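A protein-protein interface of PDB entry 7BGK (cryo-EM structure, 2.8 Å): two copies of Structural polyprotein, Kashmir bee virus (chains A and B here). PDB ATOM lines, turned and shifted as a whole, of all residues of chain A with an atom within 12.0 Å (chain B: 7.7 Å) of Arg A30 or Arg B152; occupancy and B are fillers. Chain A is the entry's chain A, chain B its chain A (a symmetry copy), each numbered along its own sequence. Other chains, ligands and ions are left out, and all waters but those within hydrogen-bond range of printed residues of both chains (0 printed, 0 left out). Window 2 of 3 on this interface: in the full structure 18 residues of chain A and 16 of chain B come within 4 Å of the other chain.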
ATOM      1  N   ASP A  19       5.302  30.092   9.634  1.00  0.00           N
ATOM      2  CA  ASP A  19       4.965  30.724   8.366  1.00  0.00           C
ATOM      3  C   ASP A  19       3.486  30.524   8.070  1.00  0.00           C
ATOM      4  O   ASP A  19       3.025  29.377   8.032  1.00  0.00           O
ATOM      5  CB  ASP A  19       5.811  30.144   7.240  1.00  0.00           C
ATOM      6  CG  ASP A  19       5.673  30.917   5.945  1.00  0.00           C
ATOM      7  OD1 ASP A  19       5.520  32.154   5.996  1.00  0.00           O
ATOM      8  OD2 ASP A  19       5.722  30.284   4.871  1.00  0.00           O
ATOM      9  N   PRO A  20       2.707  31.588   7.857  1.00  0.00           N
ATOM     10  CA  PRO A  20       1.273  31.393   7.604  1.00  0.00           C
ATOM     11  C   PRO A  20       0.977  30.639   6.327  1.00  0.00           C
ATOM     12  O   PRO A  20      -0.016  29.909   6.271  1.00  0.00           O
ATOM     13  CB  PRO A  20       0.736  32.827   7.545  1.00  0.00           C
ATOM     14  CG  PRO A  20       1.766  33.658   8.179  1.00  0.00           C
ATOM     15  CD  PRO A  20       3.056  33.015   7.877  1.00  0.00           C
ATOM     16  N   GLU A  21       1.805  30.796   5.296  1.00  0.00           N
ATOM     17  CA  GLU A  21       1.583  30.090   4.042  1.00  0.00           C
ATOM     18  C   GLU A  21       1.705  28.585   4.231  1.00  0.00           C
ATOM     19  O   GLU A  21       0.840  27.816   3.794  1.00  0.00           O
ATOM     20  CB  GLU A  21       2.573  30.613   3.001  1.00  0.00           C
ATOM     21  CG  GLU A  21       2.340  30.173   1.562  1.00  0.00           C
ATOM     22  CD  GLU A  21       3.046  28.875   1.209  1.00  0.00           C
ATOM     23  OE1 GLU A  21       4.114  28.593   1.792  1.00  0.00           O
ATOM     24  OE2 GLU A  21       2.540  28.141   0.334  1.00  0.00           O
ATOM     25  N   ARG A  22       2.761  28.147   4.915  1.00  0.00           N
ATOM     26  CA  ARG A  22       2.976  26.720   5.121  1.00  0.00           C
ATOM     27  C   ARG A  22       1.875  26.110   5.978  1.00  0.00           C
ATOM     28  O   ARG A  22       1.381  25.018   5.682  1.00  0.00           O
ATOM     29  CB  ARG A  22       4.342  26.495   5.760  1.00  0.00           C
ATOM     30  CG  ARG A  22       4.655  25.049   6.076  1.00  0.00           C
ATOM     31  CD  ARG A  22       5.941  24.908   6.854  1.00  0.00           C
ATOM     32  NE  ARG A  22       5.914  25.638   8.117  1.00  0.00           N
ATOM     33  CZ  ARG A  22       5.213  25.268   9.183  1.00  0.00           C
ATOM     34  NH1 ARG A  22       4.467  24.173   9.144  1.00  0.00           N
ATOM     35  NH2 ARG A  22       5.256  25.997  10.288  1.00  0.00           N
ATOM     36  N   MET A  23       1.482  26.802   7.046  1.00  0.00           N
ATOM     37  CA  MET A  23       0.459  26.276   7.940  1.00  0.00           C
ATOM     38  C   MET A  23      -0.905  26.261   7.269  1.00  0.00           C
ATOM     39  O   MET A  23      -1.674  25.308   7.430  1.00  0.00           O
ATOM     40  CB  MET A  23       0.426  27.106   9.213  1.00  0.00           C
ATOM     41  CG  MET A  23       1.760  27.194   9.919  1.00  0.00           C
ATOM     42  SD  MET A  23       1.985  28.728  10.815  1.00  0.00           S
ATOM     43  CE  MET A  23       1.189  28.283  12.335  1.00  0.00           C
ATOM     44  N   ASN A  24      -1.221  27.311   6.515  1.00  0.00           N
ATOM     45  CA  ASN A  24      -2.454  27.337   5.741  1.00  0.00           C
ATOM     46  C   ASN A  24      -2.509  26.186   4.752  1.00  0.00           C
ATOM     47  O   ASN A  24      -3.547  25.531   4.605  1.00  0.00           O
ATOM     48  CB  ASN A  24      -2.570  28.669   5.015  1.00  0.00           C
ATOM     49  CG  ASN A  24      -3.001  29.789   5.918  1.00  0.00           C
ATOM     50  OD1 ASN A  24      -3.362  29.573   7.070  1.00  0.00           O
ATOM     51  ND2 ASN A  24      -2.976  30.998   5.397  1.00  0.00           N
ATOM     52  N   ASN A  25      -1.406  25.935   4.047  1.00  0.00           N
ATOM     53  CA  ASN A  25      -1.359  24.807   3.129  1.00  0.00           C
ATOM     54  C   ASN A  25      -1.560  23.491   3.862  1.00  0.00           C
ATOM     55  O   ASN A  25      -2.384  22.666   3.459  1.00  0.00           O
ATOM     56  CB  ASN A  25      -0.032  24.812   2.382  1.00  0.00           C
ATOM     57  CG  ASN A  25       0.114  26.002   1.468  1.00  0.00           C
ATOM     58  OD1 ASN A  25      -0.865  26.648   1.102  1.00  0.00           O
ATOM     59  ND2 ASN A  25       1.342  26.298   1.088  1.00  0.00           N
ATOM     60  N   GLU A  26      -0.822  23.279   4.951  1.00  0.00           N
ATOM     61  CA  GLU A  26      -1.012  22.075   5.751  1.00  0.00           C
ATOM     62  C   GLU A  26      -2.471  21.895   6.138  1.00  0.00           C
ATOM     63  O   GLU A  26      -2.992  20.776   6.133  1.00  0.00           O
ATOM     64  CB  GLU A  26      -0.139  22.136   7.000  1.00  0.00           C
ATOM     65  CG  GLU A  26       1.337  21.953   6.743  1.00  0.00           C
ATOM     66  CD  GLU A  26       2.180  22.172   7.981  1.00  0.00           C
ATOM     67  OE1 GLU A  26       1.720  22.881   8.900  1.00  0.00           O
ATOM     68  OE2 GLU A  26       3.308  21.639   8.033  1.00  0.00           O
ATOM     69  N   ALA A  27      -3.147  22.990   6.478  1.00  0.00           N
ATOM     70  CA  ALA A  27      -4.545  22.905   6.878  1.00  0.00           C
ATOM     71  C   ALA A  27      -5.445  22.541   5.707  1.00  0.00           C
ATOM     72  O   ALA A  27      -6.367  21.734   5.854  1.00  0.00           O
ATOM     73  CB  ALA A  27      -4.978  24.223   7.499  1.00  0.00           C
ATOM     74  N   LEU A  28      -5.200  23.130   4.537  1.00  0.00           N
ATOM     75  CA  LEU A  28      -6.045  22.848   3.384  1.00  0.00           C
ATOM     76  C   LEU A  28      -5.856  21.429   2.877  1.00  0.00           C
ATOM     77  O   LEU A  28      -6.778  20.853   2.291  1.00  0.00           O
ATOM     78  CB  LEU A  28      -5.756  23.846   2.276  1.00  0.00           C
ATOM     79  CG  LEU A  28      -6.070  25.294   2.613  1.00  0.00           C
ATOM     80  CD1 LEU A  28      -5.404  26.169   1.624  1.00  0.00           C
ATOM     81  CD2 LEU A  28      -7.552  25.544   2.601  1.00  0.00           C
ATOM     82  N   MET A  29      -4.675  20.860   3.069  1.00  0.00           N
ATOM     83  CA  MET A  29      -4.416  19.476   2.710  1.00  0.00           C
ATOM     84  C   MET A  29      -5.032  18.493   3.689  1.00  0.00           C
ATOM     85  O   MET A  29      -4.873  17.283   3.509  1.00  0.00           O
ATOM     86  CB  MET A  29      -2.910  19.241   2.620  1.00  0.00           C
ATOM     87  CG  MET A  29      -2.172  20.229   1.750  1.00  0.00           C
ATOM     88  SD  MET A  29      -2.301  19.936  -0.010  1.00  0.00           S
ATOM     89  CE  MET A  29      -1.370  18.436  -0.128  1.00  0.00           C
ATOM     90  N   ARG A  30      -5.728  18.983   4.710  1.00  0.00           N
ATOM     91  CA  ARG A  30      -6.380  18.137   5.694  1.00  0.00           C
ATOM     92  C   ARG A  30      -7.860  18.415   5.859  1.00  0.00           C
ATOM     93  O   ARG A  30      -8.581  17.519   6.311  1.00  0.00           O
ATOM     94  CB  ARG A  30      -5.710  18.291   7.064  1.00  0.00           C
ATOM     95  CG  ARG A  30      -4.258  17.937   7.096  1.00  0.00           C
ATOM     96  CD  ARG A  30      -3.589  18.537   8.282  1.00  0.00           C
ATOM     97  NE  ARG A  30      -2.199  18.120   8.384  1.00  0.00           N
ATOM     98  CZ  ARG A  30      -1.248  18.820   8.990  1.00  0.00           C
ATOM     99  NH1 ARG A  30      -1.523  19.982   9.558  1.00  0.00           N
ATOM    100  NH2 ARG A  30      -0.013  18.351   9.027  1.00  0.00           N
ATOM    101  N   GLY A  31      -8.338  19.609   5.525  1.00  0.00           N
ATOM    102  CA  GLY A  31      -9.714  19.962   5.785  1.00  0.00           C
ATOM    103  C   GLY A  31     -10.478  20.592   4.641  1.00  0.00           C
ATOM    104  O   GLY A  31     -11.696  20.739   4.739  1.00  0.00           O
ATOM    105  N   CYS A  32      -9.798  21.005   3.572  1.00  0.00           N
ATOM    106  CA  CYS A  32     -10.483  21.549   2.403  1.00  0.00           C
ATOM    107  C   CYS A  32     -10.230  20.714   1.155  1.00  0.00           C
ATOM    108  O   CYS A  32     -11.188  20.248   0.530  1.00  0.00           O
ATOM    109  CB  CYS A  32     -10.085  23.008   2.170  1.00  0.00           C
ATOM    110  SG  CYS A  32     -11.034  23.802   0.871  1.00  0.00           S
ATOM    111  N   GLY A  33      -8.973  20.495   0.778  1.00  0.00           N
ATOM    112  CA  GLY A  33      -8.661  19.899  -0.504  1.00  0.00           C
ATOM    113  C   GLY A  33      -8.582  20.849  -1.674  1.00  0.00           C
ATOM    114  O   GLY A  33      -8.506  20.388  -2.817  1.00  0.00           O
ATOM    115  N   GLU A  34      -8.595  22.153  -1.437  1.00  0.00           N
ATOM    116  CA  GLU A  34      -8.508  23.138  -2.504  1.00  0.00           C
ATOM    117  C   GLU A  34      -8.177  24.475  -1.863  1.00  0.00           C
ATOM    118  O   GLU A  34      -8.217  24.622  -0.641  1.00  0.00           O
ATOM    119  CB  GLU A  34      -9.797  23.210  -3.324  1.00  0.00           C
ATOM    120  CG  GLU A  34     -11.076  23.289  -2.521  1.00  0.00           C
ATOM    121  CD  GLU A  34     -12.291  22.864  -3.298  1.00  0.00           C
ATOM    122  OE1 GLU A  34     -12.134  22.218  -4.350  1.00  0.00           O
ATOM    123  OE2 GLU A  34     -13.410  23.177  -2.854  1.00  0.00           O
ATOM    124  N   GLN A  35      -7.798  25.436  -2.699  1.00  0.00           N
ATOM    125  CA  GLN A  35      -7.399  26.757  -2.221  1.00  0.00           C
ATOM    126  C   GLN A  35      -7.943  27.780  -3.204  1.00  0.00           C
ATOM    127  O   GLN A  35      -7.451  27.893  -4.328  1.00  0.00           O
ATOM    128  CB  GLN A  35      -5.880  26.870  -2.058  1.00  0.00           C
ATOM    129  CG  GLN A  35      -5.304  28.274  -2.057  1.00  0.00           C
ATOM    130  CD  GLN A  35      -5.304  28.914  -0.695  1.00  0.00           C
ATOM    131  OE1 GLN A  35      -4.454  28.617   0.141  1.00  0.00           O
ATOM    132  NE2 GLN A  35      -6.265  29.798  -0.455  1.00  0.00           N
ATOM    133  N   PHE B  87     -11.352   7.424  14.872  1.00  0.00           N
ATOM    134  CA  PHE B  87     -11.282   8.611  14.039  1.00  0.00           C
ATOM    135  C   PHE B  87     -11.557   8.254  12.588  1.00  0.00           C
ATOM    136  O   PHE B  87     -11.449   7.098  12.176  1.00  0.00           O
ATOM    137  CB  PHE B  87      -9.907   9.276  14.149  1.00  0.00           C
ATOM    138  CG  PHE B  87      -9.673   9.997  15.437  1.00  0.00           C
ATOM    139  CD1 PHE B  87     -10.617  10.854  15.947  1.00  0.00           C
ATOM    140  CD2 PHE B  87      -8.495   9.824  16.128  1.00  0.00           C
ATOM    141  CE1 PHE B  87     -10.399  11.515  17.116  1.00  0.00           C
ATOM    142  CE2 PHE B  87      -8.275  10.492  17.306  1.00  0.00           C
ATOM    143  CZ  PHE B  87      -9.231  11.334  17.799  1.00  0.00           C
ATOM    144  N   TYR B  88     -11.917   9.271  11.812  1.00  0.00           N
ATOM    145  CA  TYR B  88     -11.999   9.131  10.370  1.00  0.00           C
ATOM    146  C   TYR B  88     -11.681  10.468   9.720  1.00  0.00           C
ATOM    147  O   TYR B  88     -11.716  11.520  10.359  1.00  0.00           O
ATOM    148  CB  TYR B  88     -13.367   8.612   9.917  1.00  0.00           C
ATOM    149  CG  TYR B  88     -14.499   9.610   9.940  1.00  0.00           C
ATOM    150  CD1 TYR B  88     -15.435   9.602  10.957  1.00  0.00           C
ATOM    151  CD2 TYR B  88     -14.660  10.523   8.914  1.00  0.00           C
ATOM    152  CE1 TYR B  88     -16.475  10.497  10.967  1.00  0.00           C
ATOM    153  CE2 TYR B  88     -15.693  11.418   8.916  1.00  0.00           C
ATOM    154  CZ  TYR B  88     -16.598  11.402   9.945  1.00  0.00           C
ATOM    155  OH  TYR B  88     -17.639  12.294   9.952  1.00  0.00           O
ATOM    156  N   ARG B  89     -11.350  10.406   8.435  1.00  0.00           N
ATOM    157  CA  ARG B  89     -11.097  11.595   7.642  1.00  0.00           C
ATOM    158  C   ARG B  89     -11.596  11.332   6.232  1.00  0.00           C
ATOM    159  O   ARG B  89     -11.904  10.200   5.862  1.00  0.00           O
ATOM    160  CB  ARG B  89      -9.616  11.958   7.606  1.00  0.00           C
ATOM    161  CG  ARG B  89      -8.838  11.142   6.619  1.00  0.00           C
ATOM    162  CD  ARG B  89      -7.382  11.247   6.852  1.00  0.00           C
ATOM    163  NE  ARG B  89      -6.825  12.532   6.447  1.00  0.00           N
ATOM    164  CZ  ARG B  89      -6.379  12.801   5.227  1.00  0.00           C
ATOM    165  NH1 ARG B  89      -6.444  11.896   4.265  1.00  0.00           N
ATOM    166  NH2 ARG B  89      -5.870  13.989   4.969  1.00  0.00           N
ATOM    167  N   GLY B  90     -11.658  12.393   5.448  1.00  0.00           N
ATOM    168  CA  GLY B  90     -11.997  12.293   4.050  1.00  0.00           C
ATOM    169  C   GLY B  90     -13.482  12.422   3.789  1.00  0.00           C
ATOM    170  O   GLY B  90     -14.322  12.395   4.690  1.00  0.00           O
ATOM    171  N   PHE B 147     -14.377  16.640   2.070  1.00  0.00           N
ATOM    172  CA  PHE B 147     -14.037  16.815   3.478  1.00  0.00           C
ATOM    173  C   PHE B 147     -13.843  18.300   3.721  1.00  0.00           C
ATOM    174  O   PHE B 147     -12.741  18.833   3.609  1.00  0.00           O
ATOM    175  CB  PHE B 147     -12.795  16.020   3.834  1.00  0.00           C
ATOM    176  CG  PHE B 147     -12.595  15.815   5.300  1.00  0.00           C
ATOM    177  CD1 PHE B 147     -13.577  15.243   6.079  1.00  0.00           C
ATOM    178  CD2 PHE B 147     -11.407  16.162   5.893  1.00  0.00           C
ATOM    179  CE1 PHE B 147     -13.378  15.047   7.415  1.00  0.00           C
ATOM    180  CE2 PHE B 147     -11.209  15.965   7.227  1.00  0.00           C
ATOM    181  CZ  PHE B 147     -12.193  15.406   7.987  1.00  0.00           C
ATOM    182  N   TYR B 148     -14.938  18.979   4.037  1.00  0.00           N
ATOM    183  CA  TYR B 148     -14.922  20.402   4.352  1.00  0.00           C
ATOM    184  C   TYR B 148     -15.012  20.535   5.867  1.00  0.00           C
ATOM    185  O   TYR B 148     -16.078  20.745   6.439  1.00  0.00           O
ATOM    186  CB  TYR B 148     -16.066  21.115   3.655  1.00  0.00           C
ATOM    187  CG  TYR B 148     -15.831  21.430   2.205  1.00  0.00           C
ATOM    188  CD1 TYR B 148     -14.646  21.992   1.784  1.00  0.00           C
ATOM    189  CD2 TYR B 148     -16.807  21.186   1.261  1.00  0.00           C
ATOM    190  CE1 TYR B 148     -14.436  22.293   0.470  1.00  0.00           C
ATOM    191  CE2 TYR B 148     -16.604  21.485  -0.057  1.00  0.00           C
ATOM    192  CZ  TYR B 148     -15.416  22.037  -0.447  1.00  0.00           C
ATOM    193  OH  TYR B 148     -15.200  22.345  -1.763  1.00  0.00           O
ATOM    194  N   SER B 149     -13.861  20.418   6.520  1.00  0.00           N
ATOM    195  CA  SER B 149     -13.798  20.282   7.962  1.00  0.00           C
ATOM    196  C   SER B 149     -12.964  21.389   8.588  1.00  0.00           C
ATOM    197  O   SER B 149     -12.092  21.977   7.945  1.00  0.00           O
ATOM    198  CB  SER B 149     -13.214  18.933   8.349  1.00  0.00           C
ATOM    199  OG  SER B 149     -13.204  18.757   9.748  1.00  0.00           O
ATOM    200  N   GLN B 150     -13.261  21.671   9.852  1.00  0.00           N
ATOM    201  CA  GLN B 150     -12.398  22.462  10.711  1.00  0.00           C
ATOM    202  C   GLN B 150     -11.316  21.636  11.384  1.00  0.00           C
ATOM    203  O   GLN B 150     -10.414  22.211  11.999  1.00  0.00           O
ATOM    204  CB  GLN B 150     -13.217  23.157  11.796  1.00  0.00           C
ATOM    205  CG  GLN B 150     -14.257  24.110  11.299  1.00  0.00           C
ATOM    206  CD  GLN B 150     -14.928  24.856  12.417  1.00  0.00           C
ATOM    207  OE1 GLN B 150     -14.348  25.750  13.029  1.00  0.00           O
ATOM    208  NE2 GLN B 150     -16.159  24.493  12.696  1.00  0.00           N
ATOM    209  N   TYR B 151     -11.393  20.312  11.294  1.00  0.00           N
ATOM    210  CA  TYR B 151     -10.485  19.414  11.983  1.00  0.00           C
ATOM    211  C   TYR B 151      -9.918  18.407  10.998  1.00  0.00           C
ATOM    212  O   TYR B 151     -10.558  18.054  10.007  1.00  0.00           O
ATOM    213  CB  TYR B 151     -11.192  18.685  13.118  1.00  0.00           C
ATOM    214  CG  TYR B 151     -11.957  19.596  14.040  1.00  0.00           C
ATOM    215  CD1 TYR B 151     -11.307  20.342  15.002  1.00  0.00           C
ATOM    216  CD2 TYR B 151     -13.327  19.713  13.945  1.00  0.00           C
ATOM    217  CE1 TYR B 151     -11.998  21.172  15.837  1.00  0.00           C
ATOM    218  CE2 TYR B 151     -14.025  20.543  14.780  1.00  0.00           C
ATOM    219  CZ  TYR B 151     -13.356  21.269  15.725  1.00  0.00           C
ATOM    220  OH  TYR B 151     -14.053  22.099  16.561  1.00  0.00           O
ATOM    221  N   ARG B 152      -8.701  17.949  11.285  1.00  0.00           N
ATOM    222  CA  ARG B 152      -8.023  17.004  10.412  1.00  0.00           C
ATOM    223  C   ARG B 152      -8.506  15.578  10.604  1.00  0.00           C
ATOM    224  O   ARG B 152      -8.231  14.724   9.755  1.00  0.00           O
ATOM    225  CB  ARG B 152      -6.516  17.072  10.640  1.00  0.00           C
ATOM    226  CG  ARG B 152      -6.079  16.669  12.010  1.00  0.00           C
ATOM    227  CD  ARG B 152      -4.598  16.800  12.162  1.00  0.00           C
ATOM    228  NE  ARG B 152      -4.196  18.173  12.413  1.00  0.00           N
ATOM    229  CZ  ARG B 152      -2.938  18.578  12.494  1.00  0.00           C
ATOM    230  NH1 ARG B 152      -1.949  17.717  12.341  1.00  0.00           N
ATOM    231  NH2 ARG B 152      -2.672  19.850  12.728  1.00  0.00           N
ATOM    232  N   LYS B 153      -9.210  15.303  11.695  1.00  0.00           N
ATOM    233  CA  LYS B 153      -9.773  13.990  11.953  1.00  0.00           C
ATOM    234  C   LYS B 153     -11.088  14.191  12.681  1.00  0.00           C
ATOM    235  O   LYS B 153     -11.192  15.045  13.563  1.00  0.00           O
ATOM    236  CB  LYS B 153      -8.827  13.110  12.776  1.00  0.00           C
ATOM    237  CG  LYS B 153      -8.270  13.778  14.005  1.00  0.00           C
ATOM    238  CD  LYS B 153      -7.118  13.023  14.592  1.00  0.00           C
ATOM    239  CE  LYS B 153      -6.260  13.929  15.428  1.00  0.00           C
ATOM    240  NZ  LYS B 153      -5.444  13.174  16.416  1.00  0.00           N
ATOM    241  N   ILE B 154     -12.088  13.417  12.295  1.00  0.00           N
ATOM    242  CA  ILE B 154     -13.431  13.498  12.855  1.00  0.00           C
ATOM    243  C   ILE B 154     -13.646  12.280  13.740  1.00  0.00           C
ATOM    244  O   ILE B 154     -13.385  11.157  13.297  1.00  0.00           O
ATOM    245  CB  ILE B 154     -14.509  13.563  11.759  1.00  0.00           C
ATOM    246  CG1 ILE B 154     -14.265  14.741  10.820  1.00  0.00           C
ATOM    247  CG2 ILE B 154     -15.877  13.660  12.370  1.00  0.00           C
ATOM    248  CD1 ILE B 154     -14.248  16.082  11.483  1.00  0.00           C
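The side-chain hydroxyl (OH) of Tyr B148 sits close to the side-chain carboxylate (OE2) of Glu A34 (2.3 Å).
O of Gly A31 sits close to O of Phe B147 (2.4 Å).
The guanidinium group of Arg A30 sits close to the guanidinium group of Arg B152 (3.4 Å).
The backbone carbonyl oxygen of Gly A31 sits at hydrogen-bond distance from the backbone NH of Ser B149 (2.8 Å).
O of Glu A34 lies within hydrogen-bond range of SG of Cys A32 (3.3 Å).
The backbone carbonyl oxygen (O) of Tyr B151 sits at hydrogen-bond distance from the side-chain hydroxyl (OG) of Ser B149 (2.8 Å).
Among the printed residues, pairs that only touch across the chains: Met A29 with Arg B89 (3.7 Å), Arg A30 with Phe B147 (3.2 Å), Gly A31 with Tyr B148 (3.3 Å), Cys A32 with Phe B147 (3.7 Å) and Cys A32 with Tyr B148 (3.7 Å).
Asp A19 touches none of the printed residues of chain B.
Printed residues of chain B within 4 Å of Met A29: Arg B89.
Arg A30 touches two residues of chain B.
Of the printed residues of chain B, Cys A32 touches Phe B147 and Tyr B148.
Printed residues of chain B within 4 Å of Glu A34: Tyr B148 (2.3 Å).
Arg B89 touches just one residue of chain A: Met A29.
No residue of chain A comes within 4 Å of Gly B90.
Ser B149 touches just one residue of chain A: Gly A31.
Arg B152 touches one residue of chain A.
No residue of chain A comes within 4 Å of Ile B154.
The nearest printed residue of chain A that does not touch Tyr B148 is Gly A33 (5.8 Å).
Of the 12 printed residues of chain B, 5 touch a printed residue of chain A.
Printed residues of chain B that touch a printed residue of chain A: Arg B89, Phe B147, Tyr B148, Ser B149 and Arg B152.
Hydrophobic or aromatic side chains of chain B within 4 Å of the printed part of chain A: Phe B147 and Tyr B148.
Among the printed residues, 9 pairs touch across the chains.
No position is printed for both chains.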
